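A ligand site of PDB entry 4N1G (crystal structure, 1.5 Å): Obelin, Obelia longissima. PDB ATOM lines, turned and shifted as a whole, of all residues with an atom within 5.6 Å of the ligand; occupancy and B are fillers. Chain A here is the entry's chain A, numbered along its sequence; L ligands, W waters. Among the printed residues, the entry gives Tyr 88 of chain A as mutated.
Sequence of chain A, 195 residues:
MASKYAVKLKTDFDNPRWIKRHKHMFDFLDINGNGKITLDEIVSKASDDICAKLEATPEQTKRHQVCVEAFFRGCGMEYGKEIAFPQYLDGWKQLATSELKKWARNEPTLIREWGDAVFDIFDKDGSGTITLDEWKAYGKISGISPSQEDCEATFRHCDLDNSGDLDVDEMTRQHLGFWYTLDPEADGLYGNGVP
A ring nitrogen (NE2) of His 175 sits at hydrogen-bond distance from a nitrogen (N3) of the ligand (2.9 Å). An oxygen (O3) of the ligand lies within hydrogen-bond range of a ring nitrogen (ND1) of His 22 (2.8 Å). The indole nitrogen of Trp 92 is in hydrogen-bond range of an oxygen (O3) of the ligand, at 3.5 Å. The side-chain hydroxyl (OH) of Tyr 190 sits at hydrogen-bond distance from an oxygen (O1) of the ligand (2.4 Å). OH of Tyr 88 sits at hydrogen-bond distance from O3 of the ligand.
The side-chain amino group (NZ) of Lys 45 is in hydrogen-bond range of the backbone carbonyl oxygen (O) of Phe 28, at 3.1 Å. The side-chain hydroxyl (OG) of Ser 142 lies close to the backbone NH (N) of Ile 144, at 3.5 Å. The indole nitrogen (NE1) of Trp 179 lies close to a ring nitrogen (NE2) of His 175 (3.4 Å). The indole nitrogen (NE1) of Trp 179 lies within hydrogen-bond range of the side-chain hydroxyl (OH) of Tyr 190, 2.8 Å away. NE2 of His 64 lies within hydrogen-bond range of NE1 of Trp 114, 3.1 Å away. NE1 of Trp 92 is in hydrogen-bond range of OH of Tyr 88, 3.0 Å away. The side-chain hydroxyl (OG) of Ser 142 sits at hydrogen-bond distance from the backbone carbonyl oxygen (O) of Tyr 138 (2.8 Å).
Residues that only touch the ligand: Ser 142 (3.1 Å), Trp 114 (3.2 Å), Trp 179 (3.3 Å), Met 25 (3.4 Å), Tyr 138 (3.4 Å), Gly 115 (3.5 Å), Val 118 (3.5 Å), Ile 50 (3.5 Å), Phe 72 (3.5 Å), Leu 29 (3.5 Å), Phe 28 (3.6 Å), Ala 46 (3.6 Å), Met 171 (3.7 Å) and Thr 172 (3.8 Å). Within 4 Å of the ligand: His 22, Met 25, Phe 28, Leu 29, Ala 46, Ile 50, Phe 72, Tyr 88, Trp 92, Trp 114, Gly 115, Val 118, Tyr 138, Ser 142, Met 171, Thr 172, His 175, Trp 179 and Tyr 190.
Water W1 lies within hydrogen-bond range of O2 of the ligand (2.6 Å), ND1 of His 175 (2.8 Å) and O of Ile 111 (2.9 Å). Water W2 lies within hydrogen-bond range of O of Ala 46 (2.8 Å), N1 of the ligand (3.0 Å), NE2 of His 64 (3.1 Å) and NE1 of Trp 114 (3.4 Å).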
ATOM      1  N   ARG A  21       0.267   7.000 -28.317  1.00  0.00           N
ATOM      2  CA  ARG A  21       0.446   8.376 -27.874  1.00  0.00           C
ATOM      3  C   ARG A  21       1.931   8.797 -28.002  1.00  0.00           C
ATOM      4  O   ARG A  21       2.304   9.845 -28.628  1.00  0.00           O
ATOM      5  CB  ARG A  21      -0.070   8.521 -26.427  1.00  0.00           C
ATOM      6  CG  ARG A  21       0.113   9.865 -25.804  1.00  0.00           C
ATOM      7  CD  ARG A  21      -0.818  10.043 -24.624  1.00  0.00           C
ATOM      8  NE  ARG A  21      -2.211  10.006 -25.078  1.00  0.00           N
ATOM      9  CZ  ARG A  21      -3.281  10.209 -24.309  1.00  0.00           C
ATOM     10  NH1 ARG A  21      -3.164  10.467 -23.007  1.00  0.00           N
ATOM     11  NH2 ARG A  21      -4.501  10.157 -24.868  1.00  0.00           N
ATOM     12  N   HIS A  22       2.804   7.961 -27.390  1.00  0.00           N
ATOM     13  CA  HIS A  22       4.221   8.348 -27.463  1.00  0.00           C
ATOM     14  C   HIS A  22       4.793   8.181 -28.833  1.00  0.00           C
ATOM     15  O   HIS A  22       5.745   8.919 -29.157  1.00  0.00           O
ATOM     16  CB  HIS A  22       5.063   7.569 -26.435  1.00  0.00           C
ATOM     17  CG  HIS A  22       4.803   8.016 -25.028  1.00  0.00           C
ATOM     18  ND1 HIS A  22       5.210   9.240 -24.544  1.00  0.00           N
ATOM     19  CD2 HIS A  22       4.061   7.457 -24.042  1.00  0.00           C
ATOM     20  CE1 HIS A  22       4.779   9.396 -23.306  1.00  0.00           C
ATOM     21  NE2 HIS A  22       4.092   8.317 -22.979  1.00  0.00           N
ATOM     22  N   MET A  25       4.194  11.436 -30.640  1.00  0.00           N
ATOM     23  CA  MET A  25       5.153  12.464 -30.153  1.00  0.00           C
ATOM     24  C   MET A  25       6.563  12.214 -30.679  1.00  0.00           C
ATOM     25  O   MET A  25       7.195  13.113 -31.211  1.00  0.00           O
ATOM     26  CB  MET A  25       5.143  12.481 -28.654  1.00  0.00           C
ATOM     27  CG  MET A  25       3.812  13.006 -28.103  1.00  0.00           C
ATOM     28  SD  MET A  25       3.517  14.731 -28.657  1.00  0.00           S
ATOM     29  CE  MET A  25       4.858  15.575 -27.782  1.00  0.00           C
ATOM     30  N   PHE A  26       7.021  10.978 -30.618  1.00  0.00           N
ATOM     31  CA  PHE A  26       8.338  10.604 -31.154  1.00  0.00           C
ATOM     32  C   PHE A  26       8.490  11.032 -32.606  1.00  0.00           C
ATOM     33  O   PHE A  26       9.495  11.661 -32.976  1.00  0.00           O
ATOM     34  CB  PHE A  26       8.535   9.086 -30.985  1.00  0.00           C
ATOM     35  CG  PHE A  26       9.904   8.586 -31.480  1.00  0.00           C
ATOM     36  CD1 PHE A  26      10.070   8.246 -32.778  1.00  0.00           C
ATOM     37  CD2 PHE A  26      10.979   8.433 -30.595  1.00  0.00           C
ATOM     38  CE1 PHE A  26      11.287   7.718 -33.242  1.00  0.00           C
ATOM     39  CE2 PHE A  26      12.201   7.931 -31.044  1.00  0.00           C
ATOM     40  CZ  PHE A  26      12.344   7.608 -32.393  1.00  0.00           C
ATOM     41  N   PHE A  28       6.812  13.269 -34.285  1.00  0.00           N
ATOM     42  CA  PHE A  28       6.823  14.708 -34.414  1.00  0.00           C
ATOM     43  C   PHE A  28       8.167  15.332 -33.985  1.00  0.00           C
ATOM     44  O   PHE A  28       8.670  16.273 -34.643  1.00  0.00           O
ATOM     45  CB  PHE A  28       5.715  15.315 -33.579  1.00  0.00           C
ATOM     46  CG  PHE A  28       5.573  16.794 -33.733  1.00  0.00           C
ATOM     47  CD1 PHE A  28       5.062  17.331 -34.920  1.00  0.00           C
ATOM     48  CD2 PHE A  28       5.911  17.657 -32.694  1.00  0.00           C
ATOM     49  CE1 PHE A  28       4.935  18.721 -35.091  1.00  0.00           C
ATOM     50  CE2 PHE A  28       5.796  19.065 -32.839  1.00  0.00           C
ATOM     51  CZ  PHE A  28       5.295  19.582 -34.057  1.00  0.00           C
ATOM     52  N   LEU A  29       8.760  14.823 -32.916  1.00  0.00           N
ATOM     53  CA  LEU A  29       9.976  15.410 -32.340  1.00  0.00           C
ATOM     54  C   LEU A  29      11.226  14.980 -33.154  1.00  0.00           C
ATOM     55  O   LEU A  29      12.286  15.654 -33.030  1.00  0.00           O
ATOM     56  CB  LEU A  29      10.138  15.000 -30.895  1.00  0.00           C
ATOM     57  CG  LEU A  29       9.096  15.462 -29.865  1.00  0.00           C
ATOM     58  CD1 LEU A  29       9.195  14.730 -28.541  1.00  0.00           C
ATOM     59  CD2 LEU A  29       9.239  16.945 -29.567  1.00  0.00           C
ATOM     60  N   LYS A  45      12.170  21.359 -30.024  1.00  0.00           N
ATOM     61  CA  LYS A  45      10.720  21.413 -30.235  1.00  0.00           C
ATOM     62  C   LYS A  45       9.933  21.730 -28.986  1.00  0.00           C
ATOM     63  O   LYS A  45       8.900  22.462 -29.028  1.00  0.00           O
ATOM     64  CB  LYS A  45      10.220  20.096 -30.805  1.00  0.00           C
ATOM     65  CG  LYS A  45      10.715  19.777 -32.205  1.00  0.00           C
ATOM     66  CD  LYS A  45       9.667  20.220 -33.199  1.00  0.00           C
ATOM     67  CE  LYS A  45       9.799  19.366 -34.405  1.00  0.00           C
ATOM     68  NZ  LYS A  45       8.578  19.311 -35.273  1.00  0.00           N
ATOM     69  N   ALA A  46      10.345  21.151 -27.891  1.00  0.00           N
ATOM     70  CA  ALA A  46       9.586  21.214 -26.656  1.00  0.00           C
ATOM     71  C   ALA A  46       9.948  22.463 -25.829  1.00  0.00           C
ATOM     72  O   ALA A  46       9.185  22.855 -24.901  1.00  0.00           O
ATOM     73  CB  ALA A  46       9.780  19.949 -25.806  1.00  0.00           C
ATOM     74  N   ILE A  50       8.548  26.428 -28.426  1.00  0.00           N
ATOM     75  CA  ILE A  50       7.416  26.787 -27.589  1.00  0.00           C
ATOM     76  C   ILE A  50       7.670  28.097 -26.817  1.00  0.00           C
ATOM     77  O   ILE A  50       6.782  28.954 -26.801  1.00  0.00           O
ATOM     78  CB  ILE A  50       7.092  25.627 -26.653  1.00  0.00           C
ATOM     79  CG1 ILE A  50       6.594  24.452 -27.528  1.00  0.00           C
ATOM     80  CG2 ILE A  50       6.020  26.055 -25.601  1.00  0.00           C
ATOM     81  CD1 ILE A  50       6.159  23.242 -26.713  1.00  0.00           C
ATOM     82  N   HIS A  64      12.878  26.997 -18.151  1.00  0.00           N
ATOM     83  CA  HIS A  64      12.090  26.032 -18.869  1.00  0.00           C
ATOM     84  C   HIS A  64      12.960  24.944 -19.485  1.00  0.00           C
ATOM     85  O   HIS A  64      12.749  23.824 -19.317  1.00  0.00           O
ATOM     86  CB  HIS A  64      11.235  26.720 -19.930  1.00  0.00           C
ATOM     87  CG  HIS A  64      10.298  25.782 -20.647  1.00  0.00           C
ATOM     88  ND1 HIS A  64      10.621  25.178 -21.826  1.00  0.00           N
ATOM     89  CD2 HIS A  64       9.077  25.327 -20.309  1.00  0.00           C
ATOM     90  CE1 HIS A  64       9.627  24.408 -22.212  1.00  0.00           C
ATOM     91  NE2 HIS A  64       8.671  24.498 -21.312  1.00  0.00           N
ATOM     92  N   PHE A  72      13.655  14.872 -19.579  1.00  0.00           N
ATOM     93  CA  PHE A  72      13.986  13.884 -20.574  1.00  0.00           C
ATOM     94  C   PHE A  72      15.252  13.085 -20.300  1.00  0.00           C
ATOM     95  O   PHE A  72      15.419  11.940 -20.763  1.00  0.00           O
ATOM     96  CB  PHE A  72      14.004  14.581 -21.937  1.00  0.00           C
ATOM     97  CG  PHE A  72      12.580  14.850 -22.414  1.00  0.00           C
ATOM     98  CD1 PHE A  72      11.880  13.811 -23.014  1.00  0.00           C
ATOM     99  CD2 PHE A  72      11.980  16.083 -22.243  1.00  0.00           C
ATOM    100  CE1 PHE A  72      10.513  13.984 -23.422  1.00  0.00           C
ATOM    101  CE2 PHE A  72      10.626  16.279 -22.641  1.00  0.00           C
ATOM    102  CZ  PHE A  72       9.913  15.194 -23.259  1.00  0.00           C
ATOM    103  N   TYR A  88      13.235   4.522 -26.262  1.00  0.00           N
ATOM    104  CA  TYR A  88      12.551   5.724 -25.809  1.00  0.00           C
ATOM    105  C   TYR A  88      11.355   5.362 -24.883  1.00  0.00           C
ATOM    106  O   TYR A  88      11.216   5.938 -23.775  1.00  0.00           O
ATOM    107  CB  TYR A  88      12.127   6.498 -27.063  1.00  0.00           C
ATOM    108  CG  TYR A  88      11.394   7.773 -26.762  1.00  0.00           C
ATOM    109  CD1 TYR A  88      12.076   8.929 -26.336  1.00  0.00           C
ATOM    110  CD2 TYR A  88      10.017   7.820 -26.913  1.00  0.00           C
ATOM    111  CE1 TYR A  88      11.411  10.101 -26.095  1.00  0.00           C
ATOM    112  CE2 TYR A  88       9.302   9.019 -26.661  1.00  0.00           C
ATOM    113  CZ  TYR A  88      10.000  10.134 -26.267  1.00  0.00           C
ATOM    114  OH  TYR A  88       9.270  11.284 -26.003  1.00  0.00           O
ATOM    115  N   TRP A  92      10.478   6.161 -20.901  1.00  0.00           N
ATOM    116  CA  TRP A  92       9.238   6.792 -20.402  1.00  0.00           C
ATOM    117  C   TRP A  92       8.579   5.905 -19.352  1.00  0.00           C
ATOM    118  O   TRP A  92       8.059   6.445 -18.350  1.00  0.00           O
ATOM    119  CB  TRP A  92       8.287   7.046 -21.541  1.00  0.00           C
ATOM    120  CG  TRP A  92       8.354   8.394 -22.059  1.00  0.00           C
ATOM    121  CD1 TRP A  92       9.130   8.872 -23.107  1.00  0.00           C
ATOM    122  CD2 TRP A  92       7.616   9.496 -21.561  1.00  0.00           C
ATOM    123  NE1 TRP A  92       8.902  10.238 -23.266  1.00  0.00           N
ATOM    124  CE2 TRP A  92       7.987  10.642 -22.319  1.00  0.00           C
ATOM    125  CE3 TRP A  92       6.676   9.638 -20.512  1.00  0.00           C
ATOM    126  CZ2 TRP A  92       7.431  11.911 -22.088  1.00  0.00           C
ATOM    127  CZ3 TRP A  92       6.099  10.915 -20.293  1.00  0.00           C
ATOM    128  CH2 TRP A  92       6.475  12.026 -21.099  1.00  0.00           C
ATOM    129  N   ILE A 111       7.965  16.394 -13.304  1.00  0.00           N
ATOM    130  CA  ILE A 111       6.817  16.923 -14.044  1.00  0.00           C
ATOM    131  C   ILE A 111       6.260  18.158 -13.346  1.00  0.00           C
ATOM    132  O   ILE A 111       5.912  19.135 -14.017  1.00  0.00           O
ATOM    133  CB  ILE A 111       5.760  15.820 -14.252  1.00  0.00           C
ATOM    134  CG1 ILE A 111       4.816  16.277 -15.367  1.00  0.00           C
ATOM    135  CG2 ILE A 111       5.074  15.395 -12.930  1.00  0.00           C
ATOM    136  CD1 ILE A 111       4.075  15.064 -15.929  1.00  0.00           C
ATOM    137  N   TRP A 114       8.553  21.144 -14.117  1.00  0.00           N
ATOM    138  CA  TRP A 114       8.285  21.601 -15.481  1.00  0.00           C
ATOM    139  C   TRP A 114       6.997  22.437 -15.517  1.00  0.00           C
ATOM    140  O   TRP A 114       6.966  23.526 -16.155  1.00  0.00           O
ATOM    141  CB  TRP A 114       8.210  20.397 -16.407  1.00  0.00           C
ATOM    142  CG  TRP A 114       8.151  20.719 -17.891  1.00  0.00           C
ATOM    143  CD1 TRP A 114       8.221  21.940 -18.528  1.00  0.00           C
ATOM    144  CD2 TRP A 114       8.044  19.738 -18.913  1.00  0.00           C
ATOM    145  NE1 TRP A 114       8.132  21.755 -19.900  1.00  0.00           N
ATOM    146  CE2 TRP A 114       8.038  20.424 -20.171  1.00  0.00           C
ATOM    147  CE3 TRP A 114       7.929  18.325 -18.890  1.00  0.00           C
ATOM    148  CZ2 TRP A 114       7.941  19.732 -21.422  1.00  0.00           C
ATOM    149  CZ3 TRP A 114       7.828  17.645 -20.100  1.00  0.00           C
ATOM    150  CH2 TRP A 114       7.857  18.341 -21.351  1.00  0.00           C
ATOM    151  N   GLY A 115       5.950  21.948 -14.837  1.00  0.00           N
ATOM    152  CA  GLY A 115       4.710  22.691 -14.716  1.00  0.00           C
ATOM    153  C   GLY A 115       4.922  24.104 -14.177  1.00  0.00           C
ATOM    154  O   GLY A 115       4.331  25.043 -14.682  1.00  0.00           O
ATOM    155  N   VAL A 118       6.377  26.348 -17.026  1.00  0.00           N
ATOM    156  CA  VAL A 118       5.387  26.711 -18.037  1.00  0.00           C
ATOM    157  C   VAL A 118       4.341  27.681 -17.455  1.00  0.00           C
ATOM    158  O   VAL A 118       3.954  28.692 -18.087  1.00  0.00           O
ATOM    159  CB  VAL A 118       4.718  25.461 -18.611  1.00  0.00           C
ATOM    160  CG1 VAL A 118       3.620  25.864 -19.606  1.00  0.00           C
ATOM    161  CG2 VAL A 118       5.767  24.566 -19.296  1.00  0.00           C
ATOM    162  N   PHE A 122       2.897  31.327 -18.829  1.00  0.00           N
ATOM    163  CA  PHE A 122       1.516  31.628 -19.149  1.00  0.00           C
ATOM    164  C   PHE A 122       0.934  32.771 -18.338  1.00  0.00           C
ATOM    165  O   PHE A 122       0.023  33.457 -18.785  1.00  0.00           O
ATOM    166  CB  PHE A 122       0.655  30.408 -18.863  1.00  0.00           C
ATOM    167  CG  PHE A 122       0.723  29.288 -19.881  1.00  0.00           C
ATOM    168  CD1 PHE A 122       1.380  29.387 -21.068  1.00  0.00           C
ATOM    169  CD2 PHE A 122      -0.003  28.138 -19.663  1.00  0.00           C
ATOM    170  CE1 PHE A 122       1.389  28.314 -21.965  1.00  0.00           C
ATOM    171  CE2 PHE A 122       0.006  27.083 -20.564  1.00  0.00           C
ATOM    172  CZ  PHE A 122       0.689  27.210 -21.727  1.00  0.00           C
ATOM    173  N   TYR A 138      -2.594  23.640 -26.472  1.00  0.00           N
ATOM    174  CA  TYR A 138      -1.218  23.096 -26.423  1.00  0.00           C
ATOM    175  C   TYR A 138      -0.783  22.597 -27.806  1.00  0.00           C
ATOM    176  O   TYR A 138       0.410  22.676 -28.187  1.00  0.00           O
ATOM    177  CB  TYR A 138      -1.152  21.934 -25.407  1.00  0.00           C
ATOM    178  CG  TYR A 138      -1.248  22.339 -23.944  1.00  0.00           C
ATOM    179  CD1 TYR A 138      -1.193  23.686 -23.548  1.00  0.00           C
ATOM    180  CD2 TYR A 138      -1.367  21.378 -22.980  1.00  0.00           C
ATOM    181  CE1 TYR A 138      -1.250  24.046 -22.202  1.00  0.00           C
ATOM    182  CE2 TYR A 138      -1.422  21.725 -21.645  1.00  0.00           C
ATOM    183  CZ  TYR A 138      -1.338  23.035 -21.265  1.00  0.00           C
ATOM    184  OH  TYR A 138      -1.409  23.330 -19.931  1.00  0.00           O
ATOM    185  N   SER A 142       2.440  24.176 -29.879  1.00  0.00           N
ATOM    186  CA  SER A 142       3.555  23.255 -30.130  1.00  0.00           C
ATOM    187  C   SER A 142       3.674  22.929 -31.606  1.00  0.00           C
ATOM    188  O   SER A 142       4.702  22.409 -32.030  1.00  0.00           O
ATOM    189  CB  SER A 142       3.361  21.963 -29.315  1.00  0.00           C
ATOM    190  OG  SER A 142       2.228  21.264 -29.799  1.00  0.00           O
ATOM    191  N   ILE A 144       1.889  20.659 -33.207  1.00  0.00           N
ATOM    192  CA  ILE A 144       1.551  19.280 -33.604  1.00  0.00           C
ATOM    193  C   ILE A 144       0.087  19.192 -34.064  1.00  0.00           C
ATOM    194  O   ILE A 144      -0.277  18.279 -34.840  1.00  0.00           O
ATOM    195  CB  ILE A 144       1.841  18.240 -32.463  1.00  0.00           C
ATOM    196  CG1 ILE A 144       1.831  16.810 -33.038  1.00  0.00           C
ATOM    197  CG2 ILE A 144       0.885  18.422 -31.235  1.00  0.00           C
ATOM    198  CD1 ILE A 144       2.492  15.748 -32.079  1.00  0.00           C
ATOM    199  N   MET A 171      -2.832  22.777 -13.547  1.00  0.00           N
ATOM    200  CA  MET A 171      -2.176  22.602 -14.826  1.00  0.00           C
ATOM    201  C   MET A 171      -1.298  21.306 -14.777  1.00  0.00           C
ATOM    202  O   MET A 171      -1.350  20.458 -15.691  1.00  0.00           O
ATOM    203  CB  MET A 171      -1.368  23.866 -15.144  1.00  0.00           C
ATOM    204  CG  MET A 171      -0.696  23.854 -16.505  1.00  0.00           C
ATOM    205  SD  MET A 171       0.080  25.404 -17.069  1.00  0.00           S
ATOM    206  CE  MET A 171      -1.155  26.545 -16.419  1.00  0.00           C
ATOM    207  N   THR A 172      -0.555  21.108 -13.688  1.00  0.00           N
ATOM    208  CA  THR A 172       0.333  19.965 -13.578  1.00  0.00           C
ATOM    209  C   THR A 172      -0.508  18.679 -13.523  1.00  0.00           C
ATOM    210  O   THR A 172      -0.131  17.694 -14.168  1.00  0.00           O
ATOM    211  CB  THR A 172       1.219  20.081 -12.314  1.00  0.00           C
ATOM    212  OG1 THR A 172       2.076  21.211 -12.478  1.00  0.00           O
ATOM    213  CG2 THR A 172       2.042  18.796 -12.126  1.00  0.00           C
ATOM    214  N   HIS A 175      -1.600  17.793 -17.028  1.00  0.00           N
ATOM    215  CA  HIS A 175      -0.439  17.347 -17.801  1.00  0.00           C
ATOM    216  C   HIS A 175      -0.038  15.894 -17.447  1.00  0.00           C
ATOM    217  O   HIS A 175       0.186  15.051 -18.346  1.00  0.00           O
ATOM    218  CB  HIS A 175       0.685  18.351 -17.492  1.00  0.00           C
ATOM    219  CG  HIS A 175       1.866  18.226 -18.377  1.00  0.00           C
ATOM    220  ND1 HIS A 175       3.105  17.868 -17.906  1.00  0.00           N
ATOM    221  CD2 HIS A 175       2.020  18.425 -19.719  1.00  0.00           C
ATOM    222  CE1 HIS A 175       3.977  17.839 -18.897  1.00  0.00           C
ATOM    223  NE2 HIS A 175       3.351  18.212 -20.011  1.00  0.00           N
ATOM    224  N   TRP A 179       0.105  12.425 -19.745  1.00  0.00           N
ATOM    225  CA  TRP A 179       1.359  11.741 -20.095  1.00  0.00           C
ATOM    226  C   TRP A 179       1.780  10.546 -19.230  1.00  0.00           C
ATOM    227  O   TRP A 179       2.535   9.694 -19.724  1.00  0.00           O
ATOM    228  CB  TRP A 179       2.493  12.777 -20.112  1.00  0.00           C
ATOM    229  CG  TRP A 179       2.290  13.842 -21.119  1.00  0.00           C
ATOM    230  CD1 TRP A 179       2.123  15.187 -20.868  1.00  0.00           C
ATOM    231  CD2 TRP A 179       2.221  13.669 -22.552  1.00  0.00           C
ATOM    232  NE1 TRP A 179       1.944  15.866 -22.096  1.00  0.00           N
ATOM    233  CE2 TRP A 179       1.981  14.951 -23.124  1.00  0.00           C
ATOM    234  CE3 TRP A 179       2.282  12.545 -23.400  1.00  0.00           C
ATOM    235  CZ2 TRP A 179       1.856  15.164 -24.524  1.00  0.00           C
ATOM    236  CZ3 TRP A 179       2.171  12.748 -24.796  1.00  0.00           C
ATOM    237  CH2 TRP A 179       1.963  14.059 -25.336  1.00  0.00           C
ATOM    238  N   TYR A 190      -4.038  17.776 -26.657  1.00  0.00           N
ATOM    239  CA  TYR A 190      -3.048  18.265 -27.638  1.00  0.00           C
ATOM    240  C   TYR A 190      -3.606  18.299 -29.063  1.00  0.00           C
ATOM    241  O   TYR A 190      -2.841  18.403 -30.035  1.00  0.00           O
ATOM    242  CB  TYR A 190      -1.776  17.381 -27.590  1.00  0.00           C
ATOM    243  CG  TYR A 190      -0.965  17.695 -26.337  1.00  0.00           C
ATOM    244  CD1 TYR A 190      -1.265  17.053 -25.148  1.00  0.00           C
ATOM    245  CD2 TYR A 190       0.069  18.651 -26.355  1.00  0.00           C
ATOM    246  CE1 TYR A 190      -0.547  17.329 -23.967  1.00  0.00           C
ATOM    247  CE2 TYR A 190       0.793  18.962 -25.162  1.00  0.00           C
ATOM    248  CZ  TYR A 190       0.465  18.274 -23.991  1.00  0.00           C
ATOM    249  OH  TYR A 190       1.101  18.470 -22.773  1.00  0.00           O
HETATM  250  O1  LIG L   1       2.679  20.328 -22.991  1.00  0.00           O
HETATM  251  C1  LIG L   1       3.676  21.027 -22.710  1.00  0.00           C
HETATM  252  C2  LIG L   1       3.646  22.386 -22.096  1.00  0.00           C
HETATM  253  C3  LIG L   1       3.311  22.091 -20.640  1.00  0.00           C
HETATM  254  C4  LIG L   1       4.171  21.480 -19.711  1.00  0.00           C
HETATM  255  C5  LIG L   1       3.783  21.205 -18.375  1.00  0.00           C
HETATM  256  C6  LIG L   1       2.508  21.590 -17.905  1.00  0.00           C
HETATM  257  O2  LIG L   1       2.138  21.341 -16.620  1.00  0.00           O
HETATM  258  C7  LIG L   1       1.629  22.193 -18.790  1.00  0.00           C
HETATM  259  C8  LIG L   1       2.045  22.416 -20.123  1.00  0.00           C
HETATM  260  N1  LIG L   1       4.969  20.483 -22.927  1.00  0.00           N
HETATM  261  C9  LIG L   1       5.183  19.128 -23.393  1.00  0.00           C
HETATM  262  C10 LIG L   1       5.842  18.837 -24.565  1.00  0.00           C
HETATM  263  C11 LIG L   1       6.163  19.922 -25.546  1.00  0.00           C
HETATM  264  C12 LIG L   1       5.636  19.502 -26.883  1.00  0.00           C
HETATM  265  C13 LIG L   1       6.466  19.213 -27.988  1.00  0.00           C
HETATM  266  C14 LIG L   1       5.931  18.839 -29.236  1.00  0.00           C
HETATM  267  C15 LIG L   1       4.563  18.707 -29.431  1.00  0.00           C
HETATM  268  C16 LIG L   1       3.739  18.965 -28.323  1.00  0.00           C
HETATM  269  C17 LIG L   1       4.258  19.366 -27.056  1.00  0.00           C
HETATM  270  N2  LIG L   1       6.099  17.528 -24.862  1.00  0.00           N
HETATM  271  C18 LIG L   1       5.761  16.536 -23.997  1.00  0.00           C
HETATM  272  C19 LIG L   1       5.066  16.801 -22.814  1.00  0.00           C
HETATM  273  N3  LIG L   1       4.844  18.121 -22.509  1.00  0.00           N
HETATM  274  C20 LIG L   1       6.058  15.231 -24.426  1.00  0.00           C
HETATM  275  C21 LIG L   1       7.077  14.959 -25.335  1.00  0.00           C
HETATM  276  C22 LIG L   1       7.324  13.623 -25.766  1.00  0.00           C
HETATM  277  C23 LIG L   1       6.528  12.547 -25.331  1.00  0.00           C
HETATM  278  O3  LIG L   1       6.758  11.254 -25.798  1.00  0.00           O
HETATM  279  C24 LIG L   1       5.466  12.844 -24.485  1.00  0.00           C
HETATM  280  C25 LIG L   1       5.265  14.137 -24.015  1.00  0.00           C
HETATM  281  O   HOH W   1       3.398  19.368 -15.533  1.00  0.00           O
HETATM  282  O   HOH W   2       7.038  22.598 -23.057  1.00  0.00           O
